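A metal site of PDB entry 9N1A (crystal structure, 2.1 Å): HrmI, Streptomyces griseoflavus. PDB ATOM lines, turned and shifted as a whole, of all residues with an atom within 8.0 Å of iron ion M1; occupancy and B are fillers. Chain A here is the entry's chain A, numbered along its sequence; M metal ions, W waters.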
ATOM      1  N   ASP A 165      28.905 -27.371  15.755  1.00  0.00           N
ATOM      2  CA  ASP A 165      29.390 -26.359  14.809  1.00  0.00           C
ATOM      3  C   ASP A 165      29.940 -26.910  13.489  1.00  0.00           C
ATOM      4  O   ASP A 165      29.665 -26.286  12.449  1.00  0.00           O
ATOM      5  CB  ASP A 165      30.450 -25.487  15.491  1.00  0.00           C
ATOM      6  CG  ASP A 165      29.915 -24.744  16.691  1.00  0.00           C
ATOM      7  OD1 ASP A 165      29.315 -25.388  17.577  1.00  0.00           O
ATOM      8  OD2 ASP A 165      30.071 -23.512  16.749  1.00  0.00           O
ATOM      9  N   PHE A 168      26.833 -27.256  10.946  1.00  0.00           N
ATOM     10  CA  PHE A 168      25.764 -26.262  10.835  1.00  0.00           C
ATOM     11  C   PHE A 168      25.280 -26.110   9.401  1.00  0.00           C
ATOM     12  O   PHE A 168      24.078 -25.956   9.166  1.00  0.00           O
ATOM     13  CB  PHE A 168      26.239 -24.887  11.326  1.00  0.00           C
ATOM     14  CG  PHE A 168      25.990 -24.624  12.757  1.00  0.00           C
ATOM     15  CD1 PHE A 168      25.256 -25.496  13.530  1.00  0.00           C
ATOM     16  CD2 PHE A 168      26.537 -23.496  13.363  1.00  0.00           C
ATOM     17  CE1 PHE A 168      25.043 -25.227  14.879  1.00  0.00           C
ATOM     18  CE2 PHE A 168      26.352 -23.230  14.702  1.00  0.00           C
ATOM     19  CZ  PHE A 168      25.601 -24.098  15.466  1.00  0.00           C
ATOM     20  N   ASP A 169      26.206 -26.096   8.438  1.00  0.00           N
ATOM     21  CA  ASP A 169      25.788 -25.899   7.050  1.00  0.00           C
ATOM     22  C   ASP A 169      24.794 -26.967   6.613  1.00  0.00           C
ATOM     23  O   ASP A 169      23.785 -26.657   5.950  1.00  0.00           O
ATOM     24  CB  ASP A 169      27.018 -25.839   6.102  1.00  0.00           C
ATOM     25  CG  ASP A 169      28.006 -27.010   6.295  1.00  0.00           C
ATOM     26  OD1 ASP A 169      27.733 -28.001   7.019  1.00  0.00           O
ATOM     27  OD2 ASP A 169      29.088 -26.924   5.698  1.00  0.00           O
ATOM     28  N   LEU A 172      21.377 -26.712   8.431  1.00  0.00           N
ATOM     29  CA  LEU A 172      20.546 -25.700   7.786  1.00  0.00           C
ATOM     30  C   LEU A 172      19.987 -26.214   6.475  1.00  0.00           C
ATOM     31  O   LEU A 172      18.816 -25.975   6.154  1.00  0.00           O
ATOM     32  CB  LEU A 172      21.356 -24.419   7.554  1.00  0.00           C
ATOM     33  CG  LEU A 172      21.720 -23.602   8.822  1.00  0.00           C
ATOM     34  CD1 LEU A 172      22.854 -22.649   8.562  1.00  0.00           C
ATOM     35  CD2 LEU A 172      20.505 -22.834   9.337  1.00  0.00           C
ATOM     36  N   ASN A 190      21.401 -17.661   5.656  1.00  0.00           N
ATOM     37  CA  ASN A 190      22.247 -18.180   6.714  1.00  0.00           C
ATOM     38  C   ASN A 190      23.195 -19.257   6.169  1.00  0.00           C
ATOM     39  O   ASN A 190      24.405 -19.210   6.421  1.00  0.00           O
ATOM     40  CB  ASN A 190      21.358 -18.737   7.831  1.00  0.00           C
ATOM     41  CG  ASN A 190      22.090 -18.979   9.124  1.00  0.00           C
ATOM     42  OD1 ASN A 190      23.223 -19.485   9.132  1.00  0.00           O
ATOM     43  ND2 ASN A 190      21.447 -18.640  10.248  1.00  0.00           N
ATOM     44  N   TYR A 191      22.665 -20.217   5.408  1.00  0.00           N
ATOM     45  CA  TYR A 191      23.510 -21.260   4.810  1.00  0.00           C
ATOM     46  C   TYR A 191      24.626 -20.656   3.947  1.00  0.00           C
ATOM     47  O   TYR A 191      25.796 -21.041   4.035  1.00  0.00           O
ATOM     48  CB  TYR A 191      22.650 -22.226   3.990  1.00  0.00           C
ATOM     49  CG  TYR A 191      23.425 -23.159   3.042  1.00  0.00           C
ATOM     50  CD1 TYR A 191      23.916 -24.380   3.491  1.00  0.00           C
ATOM     51  CD2 TYR A 191      23.622 -22.819   1.710  1.00  0.00           C
ATOM     52  CE1 TYR A 191      24.604 -25.243   2.637  1.00  0.00           C
ATOM     53  CE2 TYR A 191      24.337 -23.676   0.830  1.00  0.00           C
ATOM     54  CZ  TYR A 191      24.821 -24.884   1.319  1.00  0.00           C
ATOM     55  OH  TYR A 191      25.507 -25.749   0.488  1.00  0.00           O
ATOM     56  N   ASP A 193      25.995 -17.743   4.172  1.00  0.00           N
ATOM     57  CA  ASP A 193      27.029 -17.238   5.076  1.00  0.00           C
ATOM     58  C   ASP A 193      27.916 -18.373   5.601  1.00  0.00           C
ATOM     59  O   ASP A 193      29.136 -18.217   5.710  1.00  0.00           O
ATOM     60  CB  ASP A 193      26.405 -16.504   6.286  1.00  0.00           C
ATOM     61  CG  ASP A 193      25.724 -15.194   5.933  1.00  0.00           C
ATOM     62  OD1 ASP A 193      26.051 -14.570   4.903  1.00  0.00           O
ATOM     63  OD2 ASP A 193      24.859 -14.780   6.735  1.00  0.00           O
ATOM     64  N   GLU A 194      27.319 -19.506   5.961  1.00  0.00           N
ATOM     65  CA  GLU A 194      28.117 -20.646   6.434  1.00  0.00           C
ATOM     66  C   GLU A 194      29.120 -21.098   5.379  1.00  0.00           C
ATOM     67  O   GLU A 194      30.174 -21.656   5.711  1.00  0.00           O
ATOM     68  CB  GLU A 194      27.205 -21.821   6.821  1.00  0.00           C
ATOM     69  CG  GLU A 194      26.461 -21.664   8.138  1.00  0.00           C
ATOM     70  CD  GLU A 194      27.366 -21.781   9.359  1.00  0.00           C
ATOM     71  OE1 GLU A 194      28.328 -22.582   9.316  1.00  0.00           O
ATOM     72  OE2 GLU A 194      27.108 -21.059  10.351  1.00  0.00           O
ATOM     73  N   MET A 195      28.788 -20.887   4.110  1.00  0.00           N
ATOM     74  CA  MET A 195      29.687 -21.237   3.005  1.00  0.00           C
ATOM     75  C   MET A 195      30.531 -20.068   2.553  1.00  0.00           C
ATOM     76  O   MET A 195      30.884 -19.998   1.364  1.00  0.00           O
ATOM     77  CB  MET A 195      28.893 -21.810   1.839  1.00  0.00           C
ATOM     78  CG  MET A 195      27.960 -22.920   2.305  1.00  0.00           C
ATOM     79  SD  MET A 195      28.910 -24.431   2.424  1.00  0.00           S
ATOM     80  CE  MET A 195      30.186 -24.233   1.179  1.00  0.00           C
ATOM     81  N   GLU A 202      36.440 -18.142   3.996  1.00  0.00           N
ATOM     82  CA  GLU A 202      35.452 -17.718   4.975  1.00  0.00           C
ATOM     83  C   GLU A 202      34.421 -18.795   5.319  1.00  0.00           C
ATOM     84  O   GLU A 202      33.498 -18.524   6.088  1.00  0.00           O
ATOM     85  CB  GLU A 202      34.747 -16.451   4.486  1.00  0.00           C
ATOM     86  CG  GLU A 202      35.677 -15.240   4.429  1.00  0.00           C
ATOM     87  CD  GLU A 202      35.010 -14.006   3.841  1.00  0.00           C
ATOM     88  OE1 GLU A 202      33.849 -13.714   4.198  1.00  0.00           O
ATOM     89  OE2 GLU A 202      35.651 -13.312   3.024  1.00  0.00           O
ATOM     90  N   VAL A 203      34.550 -20.014   4.765  1.00  0.00           N
ATOM     91  CA  VAL A 203      33.625 -21.080   5.130  1.00  0.00           C
ATOM     92  C   VAL A 203      33.741 -21.376   6.625  1.00  0.00           C
ATOM     93  O   VAL A 203      34.839 -21.522   7.168  1.00  0.00           O
ATOM     94  CB  VAL A 203      33.906 -22.333   4.278  1.00  0.00           C
ATOM     95  CG1 VAL A 203      33.090 -23.495   4.788  1.00  0.00           C
ATOM     96  CG2 VAL A 203      33.573 -22.071   2.804  1.00  0.00           C
ATOM     97  N   HIS A 204      32.591 -21.447   7.304  1.00  0.00           N
ATOM     98  CA  HIS A 204      32.641 -21.450   8.773  1.00  0.00           C
ATOM     99  C   HIS A 204      33.259 -22.726   9.309  1.00  0.00           C
ATOM    100  O   HIS A 204      34.018 -22.683  10.288  1.00  0.00           O
ATOM    101  CB  HIS A 204      31.247 -21.246   9.362  1.00  0.00           C
ATOM    102  CG  HIS A 204      30.715 -19.877   9.137  1.00  0.00           C
ATOM    103  ND1 HIS A 204      29.542 -19.426   9.714  1.00  0.00           N
ATOM    104  CD2 HIS A 204      31.181 -18.859   8.372  1.00  0.00           C
ATOM    105  CE1 HIS A 204      29.317 -18.177   9.318  1.00  0.00           C
ATOM    106  NE2 HIS A 204      30.297 -17.817   8.506  1.00  0.00           N
ATOM    107  N   THR A 205      32.938 -23.870   8.710  1.00  0.00           N
ATOM    108  CA  THR A 205      33.527 -25.101   9.211  1.00  0.00           C
ATOM    109  C   THR A 205      35.039 -25.122   9.013  1.00  0.00           C
ATOM    110  O   THR A 205      35.765 -25.664   9.843  1.00  0.00           O
ATOM    111  CB  THR A 205      32.860 -26.309   8.562  1.00  0.00           C
ATOM    112  OG1 THR A 205      33.334 -27.503   9.195  1.00  0.00           O
ATOM    113  CG2 THR A 205      33.159 -26.374   7.073  1.00  0.00           C
ATOM    114  N   GLU A 258      21.774 -19.733  17.831  1.00  0.00           N
ATOM    115  CA  GLU A 258      22.330 -18.474  17.320  1.00  0.00           C
ATOM    116  C   GLU A 258      22.249 -17.372  18.362  1.00  0.00           C
ATOM    117  O   GLU A 258      23.177 -16.562  18.516  1.00  0.00           O
ATOM    118  CB  GLU A 258      21.592 -18.013  16.052  1.00  0.00           C
ATOM    119  CG  GLU A 258      21.426 -19.070  14.968  1.00  0.00           C
ATOM    120  CD  GLU A 258      22.725 -19.312  14.243  1.00  0.00           C
ATOM    121  OE1 GLU A 258      23.633 -19.907  14.860  1.00  0.00           O
ATOM    122  OE2 GLU A 258      22.843 -18.893  13.078  1.00  0.00           O
ATOM    123  N   VAL A 261      25.085 -17.412  21.018  1.00  0.00           N
ATOM    124  CA  VAL A 261      26.496 -17.437  20.605  1.00  0.00           C
ATOM    125  C   VAL A 261      27.232 -16.144  20.958  1.00  0.00           C
ATOM    126  O   VAL A 261      28.327 -16.225  21.530  1.00  0.00           O
ATOM    127  CB  VAL A 261      26.601 -17.786  19.110  1.00  0.00           C
ATOM    128  CG1 VAL A 261      27.882 -17.201  18.504  1.00  0.00           C
ATOM    129  CG2 VAL A 261      26.569 -19.309  18.937  1.00  0.00           C
ATOM    130  N   PHE A 265      30.591 -16.439  22.997  1.00  0.00           N
ATOM    131  CA  PHE A 265      31.857 -16.369  22.277  1.00  0.00           C
ATOM    132  C   PHE A 265      32.688 -15.156  22.702  1.00  0.00           C
ATOM    133  O   PHE A 265      33.921 -15.217  22.691  1.00  0.00           O
ATOM    134  CB  PHE A 265      31.616 -16.354  20.759  1.00  0.00           C
ATOM    135  CG  PHE A 265      31.321 -17.721  20.181  1.00  0.00           C
ATOM    136  CD1 PHE A 265      31.014 -18.787  21.020  1.00  0.00           C
ATOM    137  CD2 PHE A 265      31.366 -17.944  18.815  1.00  0.00           C
ATOM    138  CE1 PHE A 265      30.748 -20.071  20.501  1.00  0.00           C
ATOM    139  CE2 PHE A 265      31.096 -19.230  18.283  1.00  0.00           C
ATOM    140  CZ  PHE A 265      30.781 -20.288  19.139  1.00  0.00           C
ATOM    141  N   TYR A 284      37.286 -17.958  14.028  1.00  0.00           N
ATOM    142  CA  TYR A 284      35.911 -18.439  13.975  1.00  0.00           C
ATOM    143  C   TYR A 284      35.053 -17.761  15.040  1.00  0.00           C
ATOM    144  O   TYR A 284      34.028 -17.139  14.740  1.00  0.00           O
ATOM    145  CB  TYR A 284      35.867 -19.959  14.131  1.00  0.00           C
ATOM    146  CG  TYR A 284      34.468 -20.547  14.285  1.00  0.00           C
ATOM    147  CD1 TYR A 284      33.714 -20.892  13.150  1.00  0.00           C
ATOM    148  CD2 TYR A 284      33.889 -20.734  15.542  1.00  0.00           C
ATOM    149  CE1 TYR A 284      32.428 -21.408  13.276  1.00  0.00           C
ATOM    150  CE2 TYR A 284      32.605 -21.270  15.679  1.00  0.00           C
ATOM    151  CZ  TYR A 284      31.887 -21.606  14.545  1.00  0.00           C
ATOM    152  OH  TYR A 284      30.617 -22.132  14.659  1.00  0.00           O
ATOM    153  N   ALA A 287      34.707 -13.916  14.624  1.00  0.00           N
ATOM    154  CA  ALA A 287      33.777 -13.557  13.554  1.00  0.00           C
ATOM    155  C   ALA A 287      32.325 -13.769  13.975  1.00  0.00           C
ATOM    156  O   ALA A 287      31.465 -12.906  13.759  1.00  0.00           O
ATOM    157  CB  ALA A 287      34.084 -14.393  12.313  1.00  0.00           C
ATOM    158  N   HIS A 288      32.039 -14.927  14.602  1.00  0.00           N
ATOM    159  CA  HIS A 288      30.670 -15.268  14.955  1.00  0.00           C
ATOM    160  C   HIS A 288      30.056 -14.334  15.992  1.00  0.00           C
ATOM    161  O   HIS A 288      28.830 -14.301  16.103  1.00  0.00           O
ATOM    162  CB  HIS A 288      30.609 -16.720  15.432  1.00  0.00           C
ATOM    163  CG  HIS A 288      30.445 -17.670  14.298  1.00  0.00           C
ATOM    164  ND1 HIS A 288      31.403 -17.827  13.323  1.00  0.00           N
ATOM    165  CD2 HIS A 288      29.395 -18.451  13.939  1.00  0.00           C
ATOM    166  CE1 HIS A 288      30.974 -18.689  12.419  1.00  0.00           C
ATOM    167  NE2 HIS A 288      29.749 -19.084  12.769  1.00  0.00           N
ATOM    168  N   ILE A 291      28.473 -12.095  13.470  1.00  0.00           N
ATOM    169  CA  ILE A 291      27.655 -12.822  12.497  1.00  0.00           C
ATOM    170  C   ILE A 291      26.397 -13.355  13.162  1.00  0.00           C
ATOM    171  O   ILE A 291      25.279 -13.195  12.639  1.00  0.00           O
ATOM    172  CB  ILE A 291      28.453 -13.959  11.825  1.00  0.00           C
ATOM    173  CG1 ILE A 291      29.382 -13.419  10.736  1.00  0.00           C
ATOM    174  CG2 ILE A 291      27.525 -14.970  11.212  1.00  0.00           C
ATOM    175  CD1 ILE A 291      30.789 -14.034  10.756  1.00  0.00           C
ATOM    176  N   ASP A 292      26.535 -13.981  14.319  1.00  0.00           N
ATOM    177  CA  ASP A 292      25.370 -14.615  14.907  1.00  0.00           C
ATOM    178  C   ASP A 292      24.450 -13.632  15.618  1.00  0.00           C
ATOM    179  O   ASP A 292      23.294 -13.984  15.860  1.00  0.00           O
ATOM    180  CB  ASP A 292      25.805 -15.759  15.811  1.00  0.00           C
ATOM    181  CG  ASP A 292      26.037 -17.032  15.018  1.00  0.00           C
ATOM    182  OD1 ASP A 292      25.643 -17.048  13.839  1.00  0.00           O
ATOM    183  OD2 ASP A 292      26.594 -18.006  15.563  1.00  0.00           O
ATOM    184  N   HIS A 295      22.523 -13.321  12.508  1.00  0.00           N
ATOM    185  CA  HIS A 295      21.778 -14.559  12.293  1.00  0.00           C
ATOM    186  C   HIS A 295      20.619 -14.679  13.279  1.00  0.00           C
ATOM    187  O   HIS A 295      19.500 -15.036  12.880  1.00  0.00           O
ATOM    188  CB  HIS A 295      22.698 -15.775  12.402  1.00  0.00           C
ATOM    189  CG  HIS A 295      23.551 -15.993  11.201  1.00  0.00           C
ATOM    190  ND1 HIS A 295      24.489 -17.004  11.126  1.00  0.00           N
ATOM    191  CD2 HIS A 295      23.622 -15.330  10.018  1.00  0.00           C
ATOM    192  CE1 HIS A 295      25.095 -16.955   9.958  1.00  0.00           C
ATOM    193  NE2 HIS A 295      24.594 -15.945   9.267  1.00  0.00           N
HETATM  194 FE    FE M   1      28.402 -20.037  11.495  1.00  0.00          FE
HETATM  195 FE    FE M   2      25.175 -18.546  12.494  1.00  0.00          FE
HETATM  196  O   HOH W   1      25.937 -20.113  13.946  1.00  0.00           O
HETATM  197  O   HOH W   2      29.124 -21.698  12.431  1.00  0.00           O
HETATM  198  O   HOH W   3      27.040 -18.405  11.713  1.00  0.00           O
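A ring nitrogen (NE2) of His 204 is in hydrogen-bond range of the backbone carbonyl oxygen (O) of Asp 193 (3.1 Å). A ring nitrogen (ND1) of His 288 lies within hydrogen-bond range of the backbone carbonyl oxygen of Tyr 284 (3.1 Å).
Within 4 Å of iron ion M1: Glu 194, His 204 and His 288.
The side-chain carboxylate (OE2) of Glu 194 binds iron ion M1. Water W2 is bound to iron ion M1 (2.0 Å). Iron ion M1 is bound by NE2 of His 288, at 2.1 Å. Water W3 is bound to iron ion M1 (2.1 Å). Iron ion M1 is bound by a ring nitrogen (ND1) of His 204 (2.2 Å). Iron ion M1 has five donor atoms within binding distance.
Water W2 bridges OH of Tyr 284 (2.7 Å) and OE1 of Glu 194 (3.3 Å). Water W1 lies within hydrogen-bond range of OE1 of Glu 258 (2.5 Å) and OD2 of Asp 292 (2.7 Å).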
